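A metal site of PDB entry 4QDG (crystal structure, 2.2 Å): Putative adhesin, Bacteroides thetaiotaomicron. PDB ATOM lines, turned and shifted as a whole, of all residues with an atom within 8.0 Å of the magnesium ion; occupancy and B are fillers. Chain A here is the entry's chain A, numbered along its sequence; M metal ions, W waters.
Merely in contact with the magnesium ion: Asp 274 (3.4 Å) and Ser 277 (3.8 Å). Within 4 Å of the magnesium ion: Asn 151, Leu 273, Asp 274, Glu 276 and Ser 277.
The magnesium ion is bound by water W1, the backbone carbonyl oxygen (O) of Glu 276, the backbone carbonyl oxygen (O) of Leu 273 and the side-chain amide oxygen (OD1) of Asn 151. The magnesium ion has four donor atoms within binding distance.
The side-chain carboxylate of Glu 276 lies within hydrogen-bond range of the backbone NH of Glu 278. The indole nitrogen of Trp 279 sits close to the side-chain amide oxygen of Asn 151. ND2 of Asn 151 sits at hydrogen-bond distance from O of Ser 224. The backbone carbonyl oxygen (O) of Asn 151 sits at hydrogen-bond distance from the backbone NH (N) of Thr 223. The side-chain carboxylate (OD1) of Asp 274 lies within salt-bridge range of the guanidinium group (NE) of Arg 225 (2.9 Å). OD1 of Asp 274 lies within hydrogen-bond range of NE2 of Gln 270 (3.0 Å). The side-chain hydroxyl (OG) of Ser 277 sits at hydrogen-bond distance from the side-chain amino group (NZ) of Lys 148. N of Asn 152 is in hydrogen-bond range of O of Ser 277, at 2.8 Å.
Water W2 bridges the side-chain amide nitrogen of Asn 151 (2.9 Å) and the backbone NH of Leu 226 (3.0 Å).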
ATOM      1  N   TYR A  21     -10.519  -0.172  41.665  1.00  0.00           N
ATOM      2  CA  TYR A  21     -10.936  -0.317  40.266  1.00  0.00           C
ATOM      3  C   TYR A  21      -9.649  -0.521  39.451  1.00  0.00           C
ATOM      4  O   TYR A  21      -9.061   0.442  38.954  1.00  0.00           O
ATOM      5  CB  TYR A  21     -11.835   0.839  39.758  1.00  0.00           C
ATOM      6  CG  TYR A  21     -11.942   0.938  38.242  1.00  0.00           C
ATOM      7  CD1 TYR A  21     -12.400  -0.143  37.480  1.00  0.00           C
ATOM      8  CD2 TYR A  21     -11.519   2.087  37.569  1.00  0.00           C
ATOM      9  CE1 TYR A  21     -12.449  -0.069  36.076  1.00  0.00           C
ATOM     10  CE2 TYR A  21     -11.583   2.177  36.175  1.00  0.00           C
ATOM     11  CZ  TYR A  21     -12.063   1.095  35.435  1.00  0.00           C
ATOM     12  OH  TYR A  21     -12.123   1.211  34.061  1.00  0.00           O
ATOM     13  N   TYR A  23      -9.759  -3.290  37.190  1.00  0.00           N
ATOM     14  CA  TYR A  23     -10.307  -4.082  36.082  1.00  0.00           C
ATOM     15  C   TYR A  23     -10.376  -3.258  34.773  1.00  0.00           C
ATOM     16  O   TYR A  23     -11.450  -2.978  34.223  1.00  0.00           O
ATOM     17  CB  TYR A  23     -11.686  -4.640  36.427  1.00  0.00           C
ATOM     18  CG  TYR A  23     -11.971  -5.970  35.764  1.00  0.00           C
ATOM     19  CD1 TYR A  23     -11.121  -7.058  35.930  1.00  0.00           C
ATOM     20  CD2 TYR A  23     -13.132  -6.167  35.007  1.00  0.00           C
ATOM     21  CE1 TYR A  23     -11.399  -8.302  35.357  1.00  0.00           C
ATOM     22  CE2 TYR A  23     -13.420  -7.404  34.428  1.00  0.00           C
ATOM     23  CZ  TYR A  23     -12.567  -8.469  34.629  1.00  0.00           C
ATOM     24  OH  TYR A  23     -12.840  -9.695  34.082  1.00  0.00           O
ATOM     25  N   MET A 147     -15.670  -3.178  38.741  1.00  0.00           N
ATOM     26  CA  MET A 147     -15.583  -3.104  37.291  1.00  0.00           C
ATOM     27  C   MET A 147     -16.410  -1.946  36.771  1.00  0.00           C
ATOM     28  O   MET A 147     -17.286  -1.493  37.474  1.00  0.00           O
ATOM     29  CB  MET A 147     -15.971  -4.423  36.611  1.00  0.00           C
ATOM     30  CG  MET A 147     -17.441  -4.809  36.780  1.00  0.00           C
ATOM     31  SD  MET A 147     -17.901  -6.120  35.420  1.00  0.00           S
ATOM     32  CE  MET A 147     -18.404  -4.917  34.155  1.00  0.00           C
ATOM     33  N   LYS A 148     -16.103  -1.471  35.567  1.00  0.00           N
ATOM     34  CA  LYS A 148     -16.796  -0.366  34.903  1.00  0.00           C
ATOM     35  C   LYS A 148     -17.831  -0.961  33.922  1.00  0.00           C
ATOM     36  O   LYS A 148     -17.490  -1.831  33.125  1.00  0.00           O
ATOM     37  CB  LYS A 148     -15.758   0.520  34.196  1.00  0.00           C
ATOM     38  CG  LYS A 148     -16.318   1.775  33.548  1.00  0.00           C
ATOM     39  CD  LYS A 148     -15.209   2.638  33.027  1.00  0.00           C
ATOM     40  CE  LYS A 148     -15.719   3.872  32.318  1.00  0.00           C
ATOM     41  NZ  LYS A 148     -14.601   4.556  31.599  1.00  0.00           N
ATOM     42  N   ASN A 149     -19.087  -0.517  34.001  1.00  0.00           N
ATOM     43  CA  ASN A 149     -20.181  -1.020  33.153  1.00  0.00           C
ATOM     44  C   ASN A 149     -20.435  -0.170  31.922  1.00  0.00           C
ATOM     45  O   ASN A 149     -21.136  -0.625  31.026  1.00  0.00           O
ATOM     46  CB  ASN A 149     -21.507  -1.086  33.953  1.00  0.00           C
ATOM     47  CG  ASN A 149     -21.544  -2.161  35.016  1.00  0.00           C
ATOM     48  OD1 ASN A 149     -20.889  -3.190  34.914  1.00  0.00           O
ATOM     49  ND2 ASN A 149     -22.398  -1.990  36.000  1.00  0.00           N
ATOM     50  N   THR A 150     -19.940   1.089  31.891  1.00  0.00           N
ATOM     51  CA  THR A 150     -20.208   1.973  30.768  1.00  0.00           C
ATOM     52  C   THR A 150     -19.044   1.952  29.763  1.00  0.00           C
ATOM     53  O   THR A 150     -17.908   1.585  30.115  1.00  0.00           O
ATOM     54  CB  THR A 150     -20.542   3.398  31.271  1.00  0.00           C
ATOM     55  OG1 THR A 150     -19.518   3.814  32.185  1.00  0.00           O
ATOM     56  CG2 THR A 150     -21.918   3.490  31.936  1.00  0.00           C
ATOM     57  N   ASN A 151     -19.343   2.352  28.521  1.00  0.00           N
ATOM     58  CA  ASN A 151     -18.414   2.379  27.402  1.00  0.00           C
ATOM     59  C   ASN A 151     -18.577   3.610  26.560  1.00  0.00           C
ATOM     60  O   ASN A 151     -19.666   4.163  26.459  1.00  0.00           O
ATOM     61  CB  ASN A 151     -18.657   1.134  26.512  1.00  0.00           C
ATOM     62  CG  ASN A 151     -18.305  -0.158  27.167  1.00  0.00           C
ATOM     63  OD1 ASN A 151     -17.132  -0.556  27.246  1.00  0.00           O
ATOM     64  ND2 ASN A 151     -19.297  -0.798  27.726  1.00  0.00           N
ATOM     65  N   ASN A 152     -17.501   4.003  25.922  1.00  0.00           N
ATOM     66  CA  ASN A 152     -17.488   5.110  24.966  1.00  0.00           C
ATOM     67  C   ASN A 152     -16.953   4.545  23.677  1.00  0.00           C
ATOM     68  O   ASN A 152     -15.900   3.901  23.685  1.00  0.00           O
ATOM     69  CB  ASN A 152     -16.667   6.332  25.445  1.00  0.00           C
ATOM     70  CG  ASN A 152     -16.891   7.534  24.536  1.00  0.00           C
ATOM     71  OD1 ASN A 152     -17.934   8.163  24.576  1.00  0.00           O
ATOM     72  ND2 ASN A 152     -15.968   7.780  23.602  1.00  0.00           N
ATOM     73  N   THR A 223     -22.541   4.027  25.923  1.00  0.00           N
ATOM     74  CA  THR A 223     -23.489   2.931  26.132  1.00  0.00           C
ATOM     75  C   THR A 223     -23.309   2.256  27.477  1.00  0.00           C
ATOM     76  O   THR A 223     -22.325   2.484  28.190  1.00  0.00           O
ATOM     77  CB  THR A 223     -23.325   1.842  25.007  1.00  0.00           C
ATOM     78  OG1 THR A 223     -22.153   1.062  25.258  1.00  0.00           O
ATOM     79  CG2 THR A 223     -23.285   2.421  23.563  1.00  0.00           C
ATOM     80  N   SER A 224     -24.231   1.351  27.786  1.00  0.00           N
ATOM     81  CA  SER A 224     -24.165   0.536  28.981  1.00  0.00           C
ATOM     82  C   SER A 224     -23.249  -0.696  28.663  1.00  0.00           C
ATOM     83  O   SER A 224     -22.469  -0.650  27.695  1.00  0.00           O
ATOM     84  CB  SER A 224     -25.575   0.149  29.428  1.00  0.00           C
ATOM     85  OG  SER A 224     -25.605  -0.637  30.597  1.00  0.00           O
ATOM     86  N   ARG A 225     -23.320  -1.760  29.461  1.00  0.00           N
ATOM     87  CA  ARG A 225     -22.426  -2.917  29.368  1.00  0.00           C
ATOM     88  C   ARG A 225     -22.500  -3.696  28.033  1.00  0.00           C
ATOM     89  O   ARG A 225     -23.581  -4.031  27.526  1.00  0.00           O
ATOM     90  CB  ARG A 225     -22.639  -3.869  30.546  1.00  0.00           C
ATOM     91  CG  ARG A 225     -21.495  -4.815  30.789  1.00  0.00           C
ATOM     92  CD  ARG A 225     -21.746  -5.765  31.923  1.00  0.00           C
ATOM     93  NE  ARG A 225     -20.620  -6.695  32.104  1.00  0.00           N
ATOM     94  CZ  ARG A 225     -20.638  -7.726  32.939  1.00  0.00           C
ATOM     95  NH1 ARG A 225     -21.733  -7.999  33.652  1.00  0.00           N
ATOM     96  NH2 ARG A 225     -19.585  -8.517  33.053  1.00  0.00           N
ATOM     97  N   LEU A 226     -21.311  -3.977  27.487  1.00  0.00           N
ATOM     98  CA  LEU A 226     -21.114  -4.785  26.287  1.00  0.00           C
ATOM     99  C   LEU A 226     -20.878  -6.236  26.730  1.00  0.00           C
ATOM    100  O   LEU A 226     -19.921  -6.510  27.458  1.00  0.00           O
ATOM    101  CB  LEU A 226     -19.937  -4.262  25.478  1.00  0.00           C
ATOM    102  CG  LEU A 226     -20.089  -2.863  24.868  1.00  0.00           C
ATOM    103  CD1 LEU A 226     -18.749  -2.408  24.231  1.00  0.00           C
ATOM    104  CD2 LEU A 226     -21.283  -2.840  23.868  1.00  0.00           C
ATOM    105  N   MET A 227     -21.811  -7.141  26.387  1.00  0.00           N
ATOM    106  CA  MET A 227     -21.731  -8.550  26.761  1.00  0.00           C
ATOM    107  C   MET A 227     -21.982  -9.491  25.603  1.00  0.00           C
ATOM    108  O   MET A 227     -22.875  -9.254  24.805  1.00  0.00           O
ATOM    109  CB  MET A 227     -22.770  -8.898  27.859  1.00  0.00           C
ATOM    110  CG  MET A 227     -22.537  -8.193  29.175  1.00  0.00           C
ATOM    111  SD  MET A 227     -23.479  -9.034  30.655  1.00  0.00           S
ATOM    112  CE  MET A 227     -22.233 -10.613  31.034  1.00  0.00           C
ATOM    113  N   LEU A 256     -15.470  -5.999  17.675  1.00  0.00           N
ATOM    114  CA  LEU A 256     -14.497  -5.639  18.734  1.00  0.00           C
ATOM    115  C   LEU A 256     -13.655  -6.831  19.146  1.00  0.00           C
ATOM    116  O   LEU A 256     -12.487  -6.663  19.476  1.00  0.00           O
ATOM    117  CB  LEU A 256     -15.172  -5.022  19.986  1.00  0.00           C
ATOM    118  CG  LEU A 256     -16.046  -3.800  19.789  1.00  0.00           C
ATOM    119  CD1 LEU A 256     -16.727  -3.438  21.094  1.00  0.00           C
ATOM    120  CD2 LEU A 256     -15.262  -2.619  19.252  1.00  0.00           C
ATOM    121  N   GLN A 270     -15.425 -11.707  27.583  1.00  0.00           N
ATOM    122  CA  GLN A 270     -16.177 -10.821  28.491  1.00  0.00           C
ATOM    123  C   GLN A 270     -15.232  -9.887  29.275  1.00  0.00           C
ATOM    124  O   GLN A 270     -15.532  -8.702  29.409  1.00  0.00           O
ATOM    125  CB  GLN A 270     -17.080 -11.608  29.463  1.00  0.00           C
ATOM    126  CG  GLN A 270     -18.116 -10.689  30.137  1.00  0.00           C
ATOM    127  CD  GLN A 270     -18.885  -9.846  29.132  1.00  0.00           C
ATOM    128  OE1 GLN A 270     -19.555 -10.360  28.231  1.00  0.00           O
ATOM    129  NE2 GLN A 270     -18.759  -8.525  29.217  1.00  0.00           N
ATOM    130  N   GLU A 271     -14.083 -10.412  29.731  1.00  0.00           N
ATOM    131  CA  GLU A 271     -13.041  -9.642  30.447  1.00  0.00           C
ATOM    132  C   GLU A 271     -12.535  -8.482  29.591  1.00  0.00           C
ATOM    133  O   GLU A 271     -12.357  -7.387  30.107  1.00  0.00           O
ATOM    134  CB  GLU A 271     -11.878 -10.540  30.867  1.00  0.00           C
ATOM    135  CG  GLU A 271     -10.748  -9.790  31.553  1.00  0.00           C
ATOM    136  CD  GLU A 271      -9.654 -10.628  32.186  1.00  0.00           C
ATOM    137  OE1 GLU A 271      -9.687 -11.874  32.012  1.00  0.00           O
ATOM    138  OE2 GLU A 271      -8.764 -10.057  32.854  1.00  0.00           O
ATOM    139  N   PHE A 272     -12.282  -8.755  28.312  1.00  0.00           N
ATOM    140  CA  PHE A 272     -11.853  -7.774  27.314  1.00  0.00           C
ATOM    141  C   PHE A 272     -12.945  -6.708  27.149  1.00  0.00           C
ATOM    142  O   PHE A 272     -12.650  -5.495  27.180  1.00  0.00           O
ATOM    143  CB  PHE A 272     -11.561  -8.488  25.963  1.00  0.00           C
ATOM    144  CG  PHE A 272     -11.288  -7.584  24.792  1.00  0.00           C
ATOM    145  CD1 PHE A 272     -10.067  -6.930  24.678  1.00  0.00           C
ATOM    146  CD2 PHE A 272     -12.255  -7.370  23.812  1.00  0.00           C
ATOM    147  CE1 PHE A 272      -9.813  -6.070  23.591  1.00  0.00           C
ATOM    148  CE2 PHE A 272     -12.001  -6.513  22.738  1.00  0.00           C
ATOM    149  CZ  PHE A 272     -10.775  -5.889  22.633  1.00  0.00           C
ATOM    150  N   LEU A 273     -14.219  -7.145  27.017  1.00  0.00           N
ATOM    151  CA  LEU A 273     -15.340  -6.197  26.862  1.00  0.00           C
ATOM    152  C   LEU A 273     -15.577  -5.365  28.124  1.00  0.00           C
ATOM    153  O   LEU A 273     -16.072  -4.238  28.015  1.00  0.00           O
ATOM    154  CB  LEU A 273     -16.624  -6.899  26.464  1.00  0.00           C
ATOM    155  CG  LEU A 273     -16.625  -7.633  25.127  1.00  0.00           C
ATOM    156  CD1 LEU A 273     -17.818  -8.563  25.038  1.00  0.00           C
ATOM    157  CD2 LEU A 273     -16.585  -6.627  23.940  1.00  0.00           C
ATOM    158  N   ASP A 274     -15.195  -5.916  29.322  1.00  0.00           N
ATOM    159  CA  ASP A 274     -15.332  -5.172  30.577  1.00  0.00           C
ATOM    160  C   ASP A 274     -14.108  -4.330  30.873  1.00  0.00           C
ATOM    161  O   ASP A 274     -14.277  -3.185  31.264  1.00  0.00           O
ATOM    162  CB  ASP A 274     -15.618  -6.078  31.783  1.00  0.00           C
ATOM    163  CG  ASP A 274     -16.859  -6.917  31.698  1.00  0.00           C
ATOM    164  OD1 ASP A 274     -17.880  -6.401  31.200  1.00  0.00           O
ATOM    165  OD2 ASP A 274     -16.835  -8.080  32.180  1.00  0.00           O
ATOM    166  N   ARG A 275     -12.879  -4.849  30.668  1.00  0.00           N
ATOM    167  CA  ARG A 275     -11.651  -4.079  30.963  1.00  0.00           C
ATOM    168  C   ARG A 275     -11.484  -2.843  30.076  1.00  0.00           C
ATOM    169  O   ARG A 275     -10.976  -1.843  30.525  1.00  0.00           O
ATOM    170  CB  ARG A 275     -10.391  -4.945  30.829  1.00  0.00           C
ATOM    171  CG  ARG A 275     -10.165  -5.888  31.982  1.00  0.00           C
ATOM    172  CD  ARG A 275      -8.773  -6.494  31.865  1.00  0.00           C
ATOM    173  NE  ARG A 275      -8.527  -7.452  32.935  1.00  0.00           N
ATOM    174  CZ  ARG A 275      -8.034  -7.149  34.139  1.00  0.00           C
ATOM    175  NH1 ARG A 275      -7.684  -5.904  34.425  1.00  0.00           N
ATOM    176  NH2 ARG A 275      -7.869  -8.105  35.047  1.00  0.00           N
ATOM    177  N   GLU A 276     -11.859  -2.940  28.811  1.00  0.00           N
ATOM    178  CA  GLU A 276     -11.759  -1.825  27.903  1.00  0.00           C
ATOM    179  C   GLU A 276     -13.054  -1.042  27.902  1.00  0.00           C
ATOM    180  O   GLU A 276     -14.123  -1.615  27.705  1.00  0.00           O
ATOM    181  CB  GLU A 276     -11.380  -2.268  26.469  1.00  0.00           C
ATOM    182  CG  GLU A 276     -11.128  -1.087  25.537  1.00  0.00           C
ATOM    183  CD  GLU A 276     -10.035  -0.160  26.005  1.00  0.00           C
ATOM    184  OE1 GLU A 276      -8.856  -0.420  25.673  1.00  0.00           O
ATOM    185  OE2 GLU A 276     -10.342   0.830  26.720  1.00  0.00           O
ATOM    186  N   SER A 277     -12.977   0.266  28.141  1.00  0.00           N
ATOM    187  CA  SER A 277     -14.168   1.132  28.169  1.00  0.00           C
ATOM    188  C   SER A 277     -14.088   2.289  27.145  1.00  0.00           C
ATOM    189  O   SER A 277     -15.073   3.020  26.963  1.00  0.00           O
ATOM    190  CB  SER A 277     -14.372   1.682  29.581  1.00  0.00           C
ATOM    191  OG  SER A 277     -13.285   2.521  29.937  1.00  0.00           O
ATOM    192  N   GLU A 278     -12.930   2.469  26.516  1.00  0.00           N
ATOM    193  CA  GLU A 278     -12.671   3.519  25.549  1.00  0.00           C
ATOM    194  C   GLU A 278     -12.370   2.849  24.244  1.00  0.00           C
ATOM    195  O   GLU A 278     -11.369   2.150  24.144  1.00  0.00           O
ATOM    196  CB  GLU A 278     -11.541   4.470  26.010  1.00  0.00           C
ATOM    197  CG  GLU A 278     -11.881   5.328  27.223  1.00  0.00           C
ATOM    198  CD  GLU A 278     -12.974   6.388  27.085  1.00  0.00           C
ATOM    199  OE1 GLU A 278     -13.221   6.852  25.946  1.00  0.00           O
ATOM    200  OE2 GLU A 278     -13.550   6.791  28.121  1.00  0.00           O
ATOM    201  N   TRP A 279     -13.306   2.948  23.284  1.00  0.00           N
ATOM    202  CA  TRP A 279     -13.210   2.278  21.986  1.00  0.00           C
ATOM    203  C   TRP A 279     -13.198   3.252  20.849  1.00  0.00           C
ATOM    204  O   TRP A 279     -13.873   4.291  20.918  1.00  0.00           O
ATOM    205  CB  TRP A 279     -14.427   1.351  21.817  1.00  0.00           C
ATOM    206  CG  TRP A 279     -14.664   0.384  22.940  1.00  0.00           C
ATOM    207  CD1 TRP A 279     -15.495   0.557  24.012  1.00  0.00           C
ATOM    208  CD2 TRP A 279     -14.167  -0.960  23.032  1.00  0.00           C
ATOM    209  NE1 TRP A 279     -15.492  -0.563  24.799  1.00  0.00           N
ATOM    210  CE2 TRP A 279     -14.691  -1.523  24.224  1.00  0.00           C
ATOM    211  CE3 TRP A 279     -13.275  -1.727  22.256  1.00  0.00           C
ATOM    212  CZ2 TRP A 279     -14.389  -2.827  24.636  1.00  0.00           C
ATOM    213  CZ3 TRP A 279     -12.966  -3.016  22.671  1.00  0.00           C
ATOM    214  CH2 TRP A 279     -13.526  -3.545  23.847  1.00  0.00           C
HETATM  215 MG    MG M   1     -16.081  -2.103  28.624  1.00  0.00          MG
HETATM  216  O   HOH W   1     -16.573  -1.073  30.455  1.00  0.00           O
HETATM  217  O   HOH W   2     -18.681  -3.340  28.882  1.00  0.00           O
